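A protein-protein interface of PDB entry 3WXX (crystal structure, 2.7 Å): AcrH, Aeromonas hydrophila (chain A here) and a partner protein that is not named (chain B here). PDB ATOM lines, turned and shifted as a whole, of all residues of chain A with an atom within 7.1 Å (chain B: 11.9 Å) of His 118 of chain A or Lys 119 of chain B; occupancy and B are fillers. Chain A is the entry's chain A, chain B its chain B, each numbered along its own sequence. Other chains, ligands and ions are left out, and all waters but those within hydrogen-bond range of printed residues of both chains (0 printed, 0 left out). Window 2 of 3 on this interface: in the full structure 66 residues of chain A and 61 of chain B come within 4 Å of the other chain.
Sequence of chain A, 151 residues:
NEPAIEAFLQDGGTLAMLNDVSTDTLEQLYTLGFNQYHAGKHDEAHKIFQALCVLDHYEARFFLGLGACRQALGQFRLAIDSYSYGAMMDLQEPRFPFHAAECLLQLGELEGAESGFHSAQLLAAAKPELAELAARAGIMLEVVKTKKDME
OG of Ser 115 of chain A lies within hydrogen-bond range of O of Lys 119 of chain B (2.7 Å). The backbone NH (N) of Gly 122 of chain B sits at hydrogen-bond distance from the side-chain hydroxyl (OG) of Ser 115 of chain A, at 3.3 Å.
O of Ile 120 of chain B is in hydrogen-bond range of NE1 of Trp 123 of chain B (3.0 Å).
Among the printed residues, merely in contact across the chains: Pro 97 of chain A with Trp 123 of chain B (3.7 Å), Gly 112 of chain A with Trp 123 of chain B (3.6 Å), Ser 115 of chain A with Ser 118 of chain B (3.8 Å), Ser 115 of chain A with Ile 120 of chain B (3.7 Å), Ser 115 of chain A with Phe 121 of chain B (3.8 Å), Ser 115 of chain A with Trp 123 of chain B (3.6 Å), Gly 116 of chain A with Trp 123 of chain B (3.9 Å), His 118 of chain A with Lys 119 of chain B (3.99 Å) and Ser 119 of chain A with Ile 120 of chain B (3.8 Å).
Printed residues of chain B within 4 Å of Gly 112 of chain A: Trp 123. No residue of chain B comes within 4 Å of Glu 114 of chain A. Printed residues of chain B within 4 Å of Ser 115 of chain A: Ser 118 (3.8 Å), Lys 119 (2.7 Å), Ile 120 (3.7 Å), Phe 121 (3.8 Å), Gly 122 (3.3 Å) and Trp 123 (3.6 Å). Gly 116 of chain A touches just one residue of chain B: Trp 123. No residue of chain B comes within 4 Å of Phe 117 of chain A. Printed residues of chain B within 4 Å of His 118 of chain A: Lys 119. Ser 119 of chain A touches just one residue of chain B: Ile 120 (3.8 Å). No residue of chain B comes within 4 Å of Ala 120 of chain A. No residue of chain B comes within 4 Å of Gln 121 of chain A. No residue of chain B comes within 4 Å of Ala 137 of chain A. No residue of chain B comes within 4 Å of Leu 141 of chain A. Of the printed residues of chain A, Ser 118 of chain B touches Ser 115. Of the printed residues of chain A, Lys 119 of chain B touches Ser 115 and His 118. Of the printed residues of chain A, Ile 120 of chain B touches Ser 115 (3.7 Å) and Ser 119 (3.8 Å). Of the printed residues of chain A, Gly 122 of chain B touches Ser 115 (3.3 Å). Of the printed residues of chain A, Trp 123 of chain B touches Pro 97 (3.7 Å), Gly 112 (3.6 Å), Ser 115 (3.6 Å) and Gly 116 (3.9 Å). The nearest printed residue of chain A that does not touch Lys 119 of chain B is Ser 119 of chain A (4.9 Å). The nearest printed residue of chain A that does not touch Trp 123 of chain B is Ser 119 of chain A (4.6 Å).
Printed residues of chain A that touch a printed residue of chain B: Pro 97, Gly 112, Ser 115, Gly 116, His 118 and Ser 119. Hydrophobic or aromatic side chains of chain A that line the printed part of chain B: Pro 97 and His 118. Of the 18 printed residues of chain B, 6 touch a printed residue of chain A. Along chain B the printed residues that touch a printed residue of chain A span positions 118 to 123. Among the printed residues, no Asp or Glu carboxylate lies within 4 Å of a Lys or Arg side-chain nitrogen of the other chain.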
ATOM      1  N   PRO A  97     -13.556  21.485 -23.784  1.00  0.00           N
ATOM      2  CA  PRO A  97     -13.706  20.021 -23.705  1.00  0.00           C
ATOM      3  C   PRO A  97     -12.576  19.331 -22.949  1.00  0.00           C
ATOM      4  O   PRO A  97     -12.761  18.248 -22.309  1.00  0.00           O
ATOM      5  CB  PRO A  97     -13.692  19.567 -25.171  1.00  0.00           C
ATOM      6  CG  PRO A  97     -13.193  20.733 -25.945  1.00  0.00           C
ATOM      7  CD  PRO A  97     -13.539  21.968 -25.166  1.00  0.00           C
ATOM      8  N   ALA A 101     -13.186  17.211 -19.678  1.00  0.00           N
ATOM      9  CA  ALA A 101     -12.828  15.789 -19.705  1.00  0.00           C
ATOM     10  C   ALA A 101     -12.070  15.395 -18.440  1.00  0.00           C
ATOM     11  O   ALA A 101     -12.322  14.358 -17.869  1.00  0.00           O
ATOM     12  CB  ALA A 101     -12.007  15.467 -20.955  1.00  0.00           C
ATOM     13  N   GLU A 111     -17.009   7.660 -20.617  1.00  0.00           N
ATOM     14  CA  GLU A 111     -17.550   7.794 -21.958  1.00  0.00           C
ATOM     15  C   GLU A 111     -17.506   9.254 -22.340  1.00  0.00           C
ATOM     16  O   GLU A 111     -17.234   9.597 -23.481  1.00  0.00           O
ATOM     17  CB  GLU A 111     -18.980   7.257 -22.072  1.00  0.00           C
ATOM     18  CG  GLU A 111     -19.168   5.791 -21.671  1.00  0.00           C
ATOM     19  CD  GLU A 111     -19.047   5.531 -20.154  1.00  0.00           C
ATOM     20  OE1 GLU A 111     -19.301   6.449 -19.327  1.00  0.00           O
ATOM     21  OE2 GLU A 111     -18.675   4.388 -19.783  1.00  0.00           O
ATOM     22  N   GLY A 112     -17.800  10.119 -21.381  1.00  0.00           N
ATOM     23  CA  GLY A 112     -17.787  11.562 -21.625  1.00  0.00           C
ATOM     24  C   GLY A 112     -16.412  12.192 -21.523  1.00  0.00           C
ATOM     25  O   GLY A 112     -16.066  13.067 -22.309  1.00  0.00           O
ATOM     26  N   ALA A 113     -15.617  11.727 -20.563  1.00  0.00           N
ATOM     27  CA  ALA A 113     -14.183  12.032 -20.579  1.00  0.00           C
ATOM     28  C   ALA A 113     -13.614  11.764 -21.983  1.00  0.00           C
ATOM     29  O   ALA A 113     -12.904  12.585 -22.512  1.00  0.00           O
ATOM     30  CB  ALA A 113     -13.429  11.231 -19.518  1.00  0.00           C
ATOM     31  N   GLU A 114     -13.958  10.637 -22.581  1.00  0.00           N
ATOM     32  CA  GLU A 114     -13.443  10.305 -23.898  1.00  0.00           C
ATOM     33  C   GLU A 114     -13.844  11.337 -24.929  1.00  0.00           C
ATOM     34  O   GLU A 114     -13.020  11.780 -25.746  1.00  0.00           O
ATOM     35  CB  GLU A 114     -13.890   8.917 -24.366  1.00  0.00           C
ATOM     36  CG  GLU A 114     -13.282   8.563 -25.723  1.00  0.00           C
ATOM     37  CD  GLU A 114     -13.738   7.226 -26.285  1.00  0.00           C
ATOM     38  OE1 GLU A 114     -14.051   6.313 -25.501  1.00  0.00           O
ATOM     39  OE2 GLU A 114     -13.755   7.096 -27.527  1.00  0.00           O
ATOM     40  N   SER A 115     -15.109  11.704 -24.886  1.00  0.00           N
ATOM     41  CA  SER A 115     -15.647  12.660 -25.814  1.00  0.00           C
ATOM     42  C   SER A 115     -14.962  14.020 -25.708  1.00  0.00           C
ATOM     43  O   SER A 115     -14.702  14.699 -26.714  1.00  0.00           O
ATOM     44  CB  SER A 115     -17.134  12.828 -25.560  1.00  0.00           C
ATOM     45  OG  SER A 115     -17.655  13.784 -26.466  1.00  0.00           O
ATOM     46  N   GLY A 116     -14.672  14.397 -24.473  1.00  0.00           N
ATOM     47  CA  GLY A 116     -13.995  15.646 -24.179  1.00  0.00           C
ATOM     48  C   GLY A 116     -12.593  15.683 -24.698  1.00  0.00           C
ATOM     49  O   GLY A 116     -12.246  16.608 -25.427  1.00  0.00           O
ATOM     50  N   PHE A 117     -11.791  14.679 -24.322  1.00  0.00           N
ATOM     51  CA  PHE A 117     -10.402  14.598 -24.765  1.00  0.00           C
ATOM     52  C   PHE A 117     -10.319  14.473 -26.276  1.00  0.00           C
ATOM     53  O   PHE A 117      -9.419  15.062 -26.902  1.00  0.00           O
ATOM     54  CB  PHE A 117      -9.659  13.472 -24.088  1.00  0.00           C
ATOM     55  CG  PHE A 117      -9.313  13.755 -22.656  1.00  0.00           C
ATOM     56  CD1 PHE A 117      -8.721  14.948 -22.296  1.00  0.00           C
ATOM     57  CD2 PHE A 117      -9.588  12.837 -21.678  1.00  0.00           C
ATOM     58  CE1 PHE A 117      -8.467  15.232 -20.983  1.00  0.00           C
ATOM     59  CE2 PHE A 117      -9.339  13.105 -20.352  1.00  0.00           C
ATOM     60  CZ  PHE A 117      -8.768  14.300 -19.996  1.00  0.00           C
ATOM     61  N   HIS A 118     -11.280  13.752 -26.864  1.00  0.00           N
ATOM     62  CA  HIS A 118     -11.336  13.592 -28.305  1.00  0.00           C
ATOM     63  C   HIS A 118     -11.616  14.909 -29.040  1.00  0.00           C
ATOM     64  O   HIS A 118     -10.959  15.239 -30.020  1.00  0.00           O
ATOM     65  CB  HIS A 118     -12.365  12.536 -28.696  1.00  0.00           C
ATOM     66  CG  HIS A 118     -12.501  12.380 -30.173  1.00  0.00           C
ATOM     67  ND1 HIS A 118     -11.410  12.258 -31.003  1.00  0.00           N
ATOM     68  CD2 HIS A 118     -13.585  12.420 -30.978  1.00  0.00           C
ATOM     69  CE1 HIS A 118     -11.817  12.203 -32.255  1.00  0.00           C
ATOM     70  NE2 HIS A 118     -13.129  12.318 -32.269  1.00  0.00           N
ATOM     71  N   SER A 119     -12.593  15.678 -28.588  1.00  0.00           N
ATOM     72  CA  SER A 119     -12.857  16.979 -29.230  1.00  0.00           C
ATOM     73  C   SER A 119     -11.725  17.953 -28.941  1.00  0.00           C
ATOM     74  O   SER A 119     -11.388  18.798 -29.763  1.00  0.00           O
ATOM     75  CB  SER A 119     -14.192  17.555 -28.755  1.00  0.00           C
ATOM     76  OG  SER A 119     -14.250  18.960 -28.973  1.00  0.00           O
ATOM     77  N   ALA A 120     -11.163  17.871 -27.746  1.00  0.00           N
ATOM     78  CA  ALA A 120     -10.130  18.806 -27.381  1.00  0.00           C
ATOM     79  C   ALA A 120      -8.970  18.626 -28.351  1.00  0.00           C
ATOM     80  O   ALA A 120      -8.399  19.612 -28.803  1.00  0.00           O
ATOM     81  CB  ALA A 120      -9.678  18.595 -25.954  1.00  0.00           C
ATOM     82  N   GLN A 121      -8.666  17.374 -28.701  1.00  0.00           N
ATOM     83  CA  GLN A 121      -7.601  17.101 -29.650  1.00  0.00           C
ATOM     84  C   GLN A 121      -7.870  17.688 -31.033  1.00  0.00           C
ATOM     85  O   GLN A 121      -7.016  18.367 -31.602  1.00  0.00           O
ATOM     86  CB  GLN A 121      -7.358  15.607 -29.789  1.00  0.00           C
ATOM     87  CG  GLN A 121      -6.436  15.248 -30.964  1.00  0.00           C
ATOM     88  CD  GLN A 121      -5.798  13.902 -30.767  1.00  0.00           C
ATOM     89  OE1 GLN A 121      -4.589  13.806 -30.544  1.00  0.00           O
ATOM     90  NE2 GLN A 121      -6.619  12.843 -30.797  1.00  0.00           N
ATOM     91  N   LEU A 122      -9.032  17.385 -31.591  1.00  0.00           N
ATOM     92  CA  LEU A 122      -9.389  17.911 -32.902  1.00  0.00           C
ATOM     93  C   LEU A 122      -9.225  19.420 -32.947  1.00  0.00           C
ATOM     94  O   LEU A 122      -8.606  19.965 -33.854  1.00  0.00           O
ATOM     95  CB  LEU A 122     -10.829  17.520 -33.251  1.00  0.00           C
ATOM     96  CG  LEU A 122     -11.114  16.013 -33.372  1.00  0.00           C
ATOM     97  CD1 LEU A 122     -12.603  15.725 -33.511  1.00  0.00           C
ATOM     98  CD2 LEU A 122     -10.350  15.440 -34.556  1.00  0.00           C
ATOM     99  N   LEU A 123      -9.817  20.110 -31.980  1.00  0.00           N
ATOM    100  CA  LEU A 123      -9.854  21.571 -31.998  1.00  0.00           C
ATOM    101  C   LEU A 123      -8.476  22.164 -31.785  1.00  0.00           C
ATOM    102  O   LEU A 123      -8.134  23.183 -32.386  1.00  0.00           O
ATOM    103  CB  LEU A 123     -10.800  22.090 -30.907  1.00  0.00           C
ATOM    104  CG  LEU A 123     -12.282  21.764 -31.076  1.00  0.00           C
ATOM    105  CD1 LEU A 123     -13.031  22.057 -29.771  1.00  0.00           C
ATOM    106  CD2 LEU A 123     -12.852  22.570 -32.228  1.00  0.00           C
ATOM    107  N   ALA A 137      -4.059  16.068 -25.031  1.00  0.00           N
ATOM    108  CA  ALA A 137      -5.399  15.572 -25.252  1.00  0.00           C
ATOM    109  C   ALA A 137      -5.306  14.163 -25.816  1.00  0.00           C
ATOM    110  O   ALA A 137      -5.965  13.238 -25.323  1.00  0.00           O
ATOM    111  CB  ALA A 137      -6.165  16.486 -26.185  1.00  0.00           C
ATOM    112  N   GLY A 138      -4.439  13.995 -26.802  1.00  0.00           N
ATOM    113  CA  GLY A 138      -4.199  12.680 -27.394  1.00  0.00           C
ATOM    114  C   GLY A 138      -3.801  11.655 -26.369  1.00  0.00           C
ATOM    115  O   GLY A 138      -4.280  10.529 -26.406  1.00  0.00           O
ATOM    116  N   MET A 140      -4.337  11.671 -23.012  1.00  0.00           N
ATOM    117  CA  MET A 140      -5.407  11.419 -22.038  1.00  0.00           C
ATOM    118  C   MET A 140      -6.513  10.654 -22.692  1.00  0.00           C
ATOM    119  O   MET A 140      -7.162   9.811 -22.075  1.00  0.00           O
ATOM    120  CB  MET A 140      -5.967  12.733 -21.512  1.00  0.00           C
ATOM    121  CG  MET A 140      -4.983  13.545 -20.692  1.00  0.00           C
ATOM    122  SD  MET A 140      -4.322  12.471 -19.165  1.00  0.00           S
ATOM    123  CE  MET A 140      -5.974  12.019 -18.186  1.00  0.00           C
ATOM    124  N   LEU A 141      -6.727  10.933 -23.963  1.00  0.00           N
ATOM    125  CA  LEU A 141      -7.637  10.123 -24.745  1.00  0.00           C
ATOM    126  C   LEU A 141      -7.294   8.635 -24.624  1.00  0.00           C
ATOM    127  O   LEU A 141      -8.165   7.844 -24.263  1.00  0.00           O
ATOM    128  CB  LEU A 141      -7.633  10.566 -26.197  1.00  0.00           C
ATOM    129  CG  LEU A 141      -8.567   9.823 -27.130  1.00  0.00           C
ATOM    130  CD1 LEU A 141      -9.967   9.678 -26.571  1.00  0.00           C
ATOM    131  CD2 LEU A 141      -8.635  10.590 -28.439  1.00  0.00           C
ATOM    132  N   ALA B 107     -24.515  24.533 -34.550  1.00  0.00           N
ATOM    133  CA  ALA B 107     -23.660  23.438 -34.080  1.00  0.00           C
ATOM    134  C   ALA B 107     -24.479  22.337 -33.454  1.00  0.00           C
ATOM    135  O   ALA B 107     -24.212  21.175 -33.661  1.00  0.00           O
ATOM    136  CB  ALA B 107     -22.625  23.948 -33.088  1.00  0.00           C
ATOM    137  N   ALA B 108     -25.467  22.703 -32.663  1.00  0.00           N
ATOM    138  CA  ALA B 108     -26.313  21.709 -32.021  1.00  0.00           C
ATOM    139  C   ALA B 108     -27.236  21.054 -33.040  1.00  0.00           C
ATOM    140  O   ALA B 108     -27.541  19.872 -32.920  1.00  0.00           O
ATOM    141  CB  ALA B 108     -27.119  22.344 -30.901  1.00  0.00           C
ATOM    142  N   LYS B 110     -26.692  20.590 -36.452  1.00  0.00           N
ATOM    143  CA  LYS B 110     -25.885  19.682 -37.264  1.00  0.00           C
ATOM    144  C   LYS B 110     -25.329  18.490 -36.475  1.00  0.00           C
ATOM    145  O   LYS B 110     -24.942  17.481 -37.065  1.00  0.00           O
ATOM    146  CB  LYS B 110     -24.809  20.466 -38.061  1.00  0.00           C
ATOM    147  CG  LYS B 110     -23.358  20.004 -37.918  1.00  0.00           C
ATOM    148  CD  LYS B 110     -22.421  20.627 -38.954  1.00  0.00           C
ATOM    149  CE  LYS B 110     -21.326  19.624 -39.287  1.00  0.00           C
ATOM    150  NZ  LYS B 110     -20.317  20.165 -40.230  1.00  0.00           N
ATOM    151  N   ALA B 111     -25.312  18.579 -35.153  1.00  0.00           N
ATOM    152  CA  ALA B 111     -24.808  17.483 -34.327  1.00  0.00           C
ATOM    153  C   ALA B 111     -25.880  16.419 -34.105  1.00  0.00           C
ATOM    154  O   ALA B 111     -25.590  15.236 -34.042  1.00  0.00           O
ATOM    155  CB  ALA B 111     -24.292  18.021 -32.995  1.00  0.00           C
ATOM    156  N   LYS B 112     -27.120  16.853 -33.966  1.00  0.00           N
ATOM    157  CA  LYS B 112     -28.229  15.973 -33.679  1.00  0.00           C
ATOM    158  C   LYS B 112     -28.784  15.290 -34.942  1.00  0.00           C
ATOM    159  O   LYS B 112     -29.493  14.287 -34.837  1.00  0.00           O
ATOM    160  CB  LYS B 112     -29.273  16.874 -32.971  1.00  0.00           C
ATOM    161  CG  LYS B 112     -30.676  16.368 -32.642  1.00  0.00           C
ATOM    162  CD  LYS B 112     -31.765  16.961 -33.549  1.00  0.00           C
ATOM    163  CE  LYS B 112     -33.044  16.119 -33.560  1.00  0.00           C
ATOM    164  NZ  LYS B 112     -34.252  16.929 -33.897  1.00  0.00           N
ATOM    165  N   LYS B 113     -28.440  15.803 -36.125  1.00  0.00           N
ATOM    166  CA  LYS B 113     -28.771  15.128 -37.383  1.00  0.00           C
ATOM    167  C   LYS B 113     -27.770  14.003 -37.582  1.00  0.00           C
ATOM    168  O   LYS B 113     -28.147  12.831 -37.625  1.00  0.00           O
ATOM    169  CB  LYS B 113     -28.741  16.083 -38.582  1.00  0.00           C
ATOM    170  CG  LYS B 113     -29.649  17.290 -38.456  1.00  0.00           C
ATOM    171  CD  LYS B 113     -29.568  18.184 -39.672  1.00  0.00           C
ATOM    172  CE  LYS B 113     -30.494  19.392 -39.609  1.00  0.00           C
ATOM    173  NZ  LYS B 113     -30.334  20.258 -40.810  1.00  0.00           N
ATOM    174  N   SER B 114     -26.491  14.365 -37.669  1.00  0.00           N
ATOM    175  CA  SER B 114     -25.402  13.403 -37.772  1.00  0.00           C
ATOM    176  C   SER B 114     -25.385  12.413 -36.588  1.00  0.00           C
ATOM    177  O   SER B 114     -26.004  12.643 -35.543  1.00  0.00           O
ATOM    178  CB  SER B 114     -24.068  14.171 -37.909  1.00  0.00           C
ATOM    179  OG  SER B 114     -22.979  13.417 -37.444  1.00  0.00           O
ATOM    180  N   GLY B 115     -24.702  11.288 -36.780  1.00  0.00           N
ATOM    181  CA  GLY B 115     -24.468  10.333 -35.699  1.00  0.00           C
ATOM    182  C   GLY B 115     -23.323  10.746 -34.786  1.00  0.00           C
ATOM    183  O   GLY B 115     -22.985  10.012 -33.863  1.00  0.00           O
ATOM    184  N   LEU B 116     -22.732  11.922 -35.032  1.00  0.00           N
ATOM    185  CA  LEU B 116     -21.605  12.431 -34.231  1.00  0.00           C
ATOM    186  C   LEU B 116     -22.089  13.430 -33.140  1.00  0.00           C
ATOM    187  O   LEU B 116     -21.395  14.401 -32.779  1.00  0.00           O
ATOM    188  CB  LEU B 116     -20.503  13.025 -35.136  1.00  0.00           C
ATOM    189  CG  LEU B 116     -19.742  12.250 -36.200  1.00  0.00           C
ATOM    190  CD1 LEU B 116     -20.594  11.285 -36.998  1.00  0.00           C
ATOM    191  CD2 LEU B 116     -19.047  13.239 -37.128  1.00  0.00           C
ATOM    192  N   ALA B 117     -23.284  13.160 -32.605  1.00  0.00           N
ATOM    193  CA  ALA B 117     -23.830  13.925 -31.489  1.00  0.00           C
ATOM    194  C   ALA B 117     -22.932  13.753 -30.261  1.00  0.00           C
ATOM    195  O   ALA B 117     -22.166  14.657 -29.933  1.00  0.00           O
ATOM    196  CB  ALA B 117     -25.268  13.500 -31.188  1.00  0.00           C
ATOM    197  N   SER B 118     -22.984  12.583 -29.619  1.00  0.00           N
ATOM    198  CA  SER B 118     -22.232  12.329 -28.376  1.00  0.00           C
ATOM    199  C   SER B 118     -20.774  11.922 -28.598  1.00  0.00           C
ATOM    200  O   SER B 118     -20.206  11.209 -27.761  1.00  0.00           O
ATOM    201  CB  SER B 118     -22.902  11.214 -27.549  1.00  0.00           C
ATOM    202  OG  SER B 118     -24.313  11.289 -27.592  1.00  0.00           O
ATOM    203  N   LYS B 119     -20.180  12.348 -29.714  1.00  0.00           N
ATOM    204  CA  LYS B 119     -18.751  12.149 -29.951  1.00  0.00           C
ATOM    205  C   LYS B 119     -17.948  13.415 -29.704  1.00  0.00           C
ATOM    206  O   LYS B 119     -16.922  13.372 -29.018  1.00  0.00           O
ATOM    207  CB  LYS B 119     -18.484  11.566 -31.346  1.00  0.00           C
ATOM    208  CG  LYS B 119     -18.246  10.078 -31.149  1.00  0.00           C
ATOM    209  CD  LYS B 119     -17.601   9.247 -32.254  1.00  0.00           C
ATOM    210  CE  LYS B 119     -16.981   7.980 -31.690  1.00  0.00           C
ATOM    211  NZ  LYS B 119     -16.897   6.874 -32.681  1.00  0.00           N
ATOM    212  N   ILE B 120     -18.419  14.535 -30.245  1.00  0.00           N
ATOM    213  CA  ILE B 120     -17.813  15.829 -29.911  1.00  0.00           C
ATOM    214  C   ILE B 120     -18.553  16.586 -28.789  1.00  0.00           C
ATOM    215  O   ILE B 120     -17.960  17.493 -28.187  1.00  0.00           O
ATOM    216  CB  ILE B 120     -17.626  16.756 -31.141  1.00  0.00           C
ATOM    217  CG1 ILE B 120     -18.928  16.887 -31.940  1.00  0.00           C
ATOM    218  CG2 ILE B 120     -16.455  16.280 -32.003  1.00  0.00           C
ATOM    219  CD1 ILE B 120     -18.967  18.136 -32.794  1.00  0.00           C
ATOM    220  N   PHE B 121     -19.815  16.224 -28.506  1.00  0.00           N
ATOM    221  CA  PHE B 121     -20.629  16.924 -27.487  1.00  0.00           C
ATOM    222  C   PHE B 121     -21.234  16.027 -26.411  1.00  0.00           C
ATOM    223  O   PHE B 121     -22.079  16.463 -25.644  1.00  0.00           O
ATOM    224  CB  PHE B 121     -21.714  17.778 -28.148  1.00  0.00           C
ATOM    225  CG  PHE B 121     -21.170  18.929 -28.945  1.00  0.00           C
ATOM    226  CD1 PHE B 121     -20.378  19.876 -28.356  1.00  0.00           C
ATOM    227  CD2 PHE B 121     -21.454  19.061 -30.299  1.00  0.00           C
ATOM    228  CE1 PHE B 121     -19.881  20.943 -29.086  1.00  0.00           C
ATOM    229  CE2 PHE B 121     -20.945  20.124 -31.050  1.00  0.00           C
ATOM    230  CZ  PHE B 121     -20.152  21.067 -30.439  1.00  0.00           C
ATOM    231  N   GLY B 122     -20.743  14.804 -26.295  1.00  0.00           N
ATOM    232  CA  GLY B 122     -21.193  13.907 -25.240  1.00  0.00           C
ATOM    233  C   GLY B 122     -20.713  14.336 -23.880  1.00  0.00           C
ATOM    234  O   GLY B 122     -21.217  13.880 -22.852  1.00  0.00           O
ATOM    235  N   TRP B 123     -19.722  15.218 -23.867  1.00  0.00           N
ATOM    236  CA  TRP B 123     -19.165  15.730 -22.606  1.00  0.00           C
ATOM    237  C   TRP B 123     -20.036  16.837 -22.011  1.00  0.00           C
ATOM    238  O   TRP B 123     -20.010  17.096 -20.813  1.00  0.00           O
ATOM    239  CB  TRP B 123     -17.722  16.210 -22.816  1.00  0.00           C
ATOM    240  CG  TRP B 123     -17.538  17.365 -23.693  1.00  0.00           C
ATOM    241  CD1 TRP B 123     -17.364  17.353 -25.042  1.00  0.00           C
ATOM    242  CD2 TRP B 123     -17.518  18.719 -23.300  1.00  0.00           C
ATOM    243  NE1 TRP B 123     -17.242  18.632 -25.529  1.00  0.00           N
ATOM    244  CE2 TRP B 123     -17.335  19.496 -24.470  1.00  0.00           C
ATOM    245  CE3 TRP B 123     -17.693  19.372 -22.080  1.00  0.00           C
ATOM    246  CZ2 TRP B 123     -17.276  20.889 -24.435  1.00  0.00           C
ATOM    247  CZ3 TRP B 123     -17.654  20.759 -22.051  1.00  0.00           C
ATOM    248  CH2 TRP B 123     -17.442  21.498 -23.224  1.00  0.00           C
ATOM    249  N   ILE B 124     -20.827  17.466 -22.855  1.00  0.00           N
ATOM    250  CA  ILE B 124     -21.690  18.562 -22.417  1.00  0.00           C
ATOM    251  C   ILE B 124     -22.687  18.133 -21.334  1.00  0.00           C
ATOM    252  O   ILE B 124     -23.295  17.094 -21.419  1.00  0.00           O
ATOM    253  CB  ILE B 124     -22.318  19.177 -23.657  1.00  0.00           C
ATOM    254  CG1 ILE B 124     -21.254  20.039 -24.296  1.00  0.00           C
ATOM    255  CG2 ILE B 124     -23.543  19.972 -23.333  1.00  0.00           C
ATOM    256  CD1 ILE B 124     -21.755  20.879 -25.439  1.00  0.00           C
ATOM    257  N   SER B 125     -22.803  18.892 -20.274  1.00  0.00           N
ATOM    258  CA  SER B 125     -23.645  18.453 -19.151  1.00  0.00           C
ATOM    259  C   SER B 125     -25.097  18.558 -19.548  1.00  0.00           C
ATOM    260  O   SER B 125     -25.441  19.233 -20.540  1.00  0.00           O
ATOM    261  CB  SER B 125     -23.427  19.320 -17.905  1.00  0.00           C
ATOM    262  OG  SER B 125     -23.675  20.690 -18.173  1.00  0.00           O
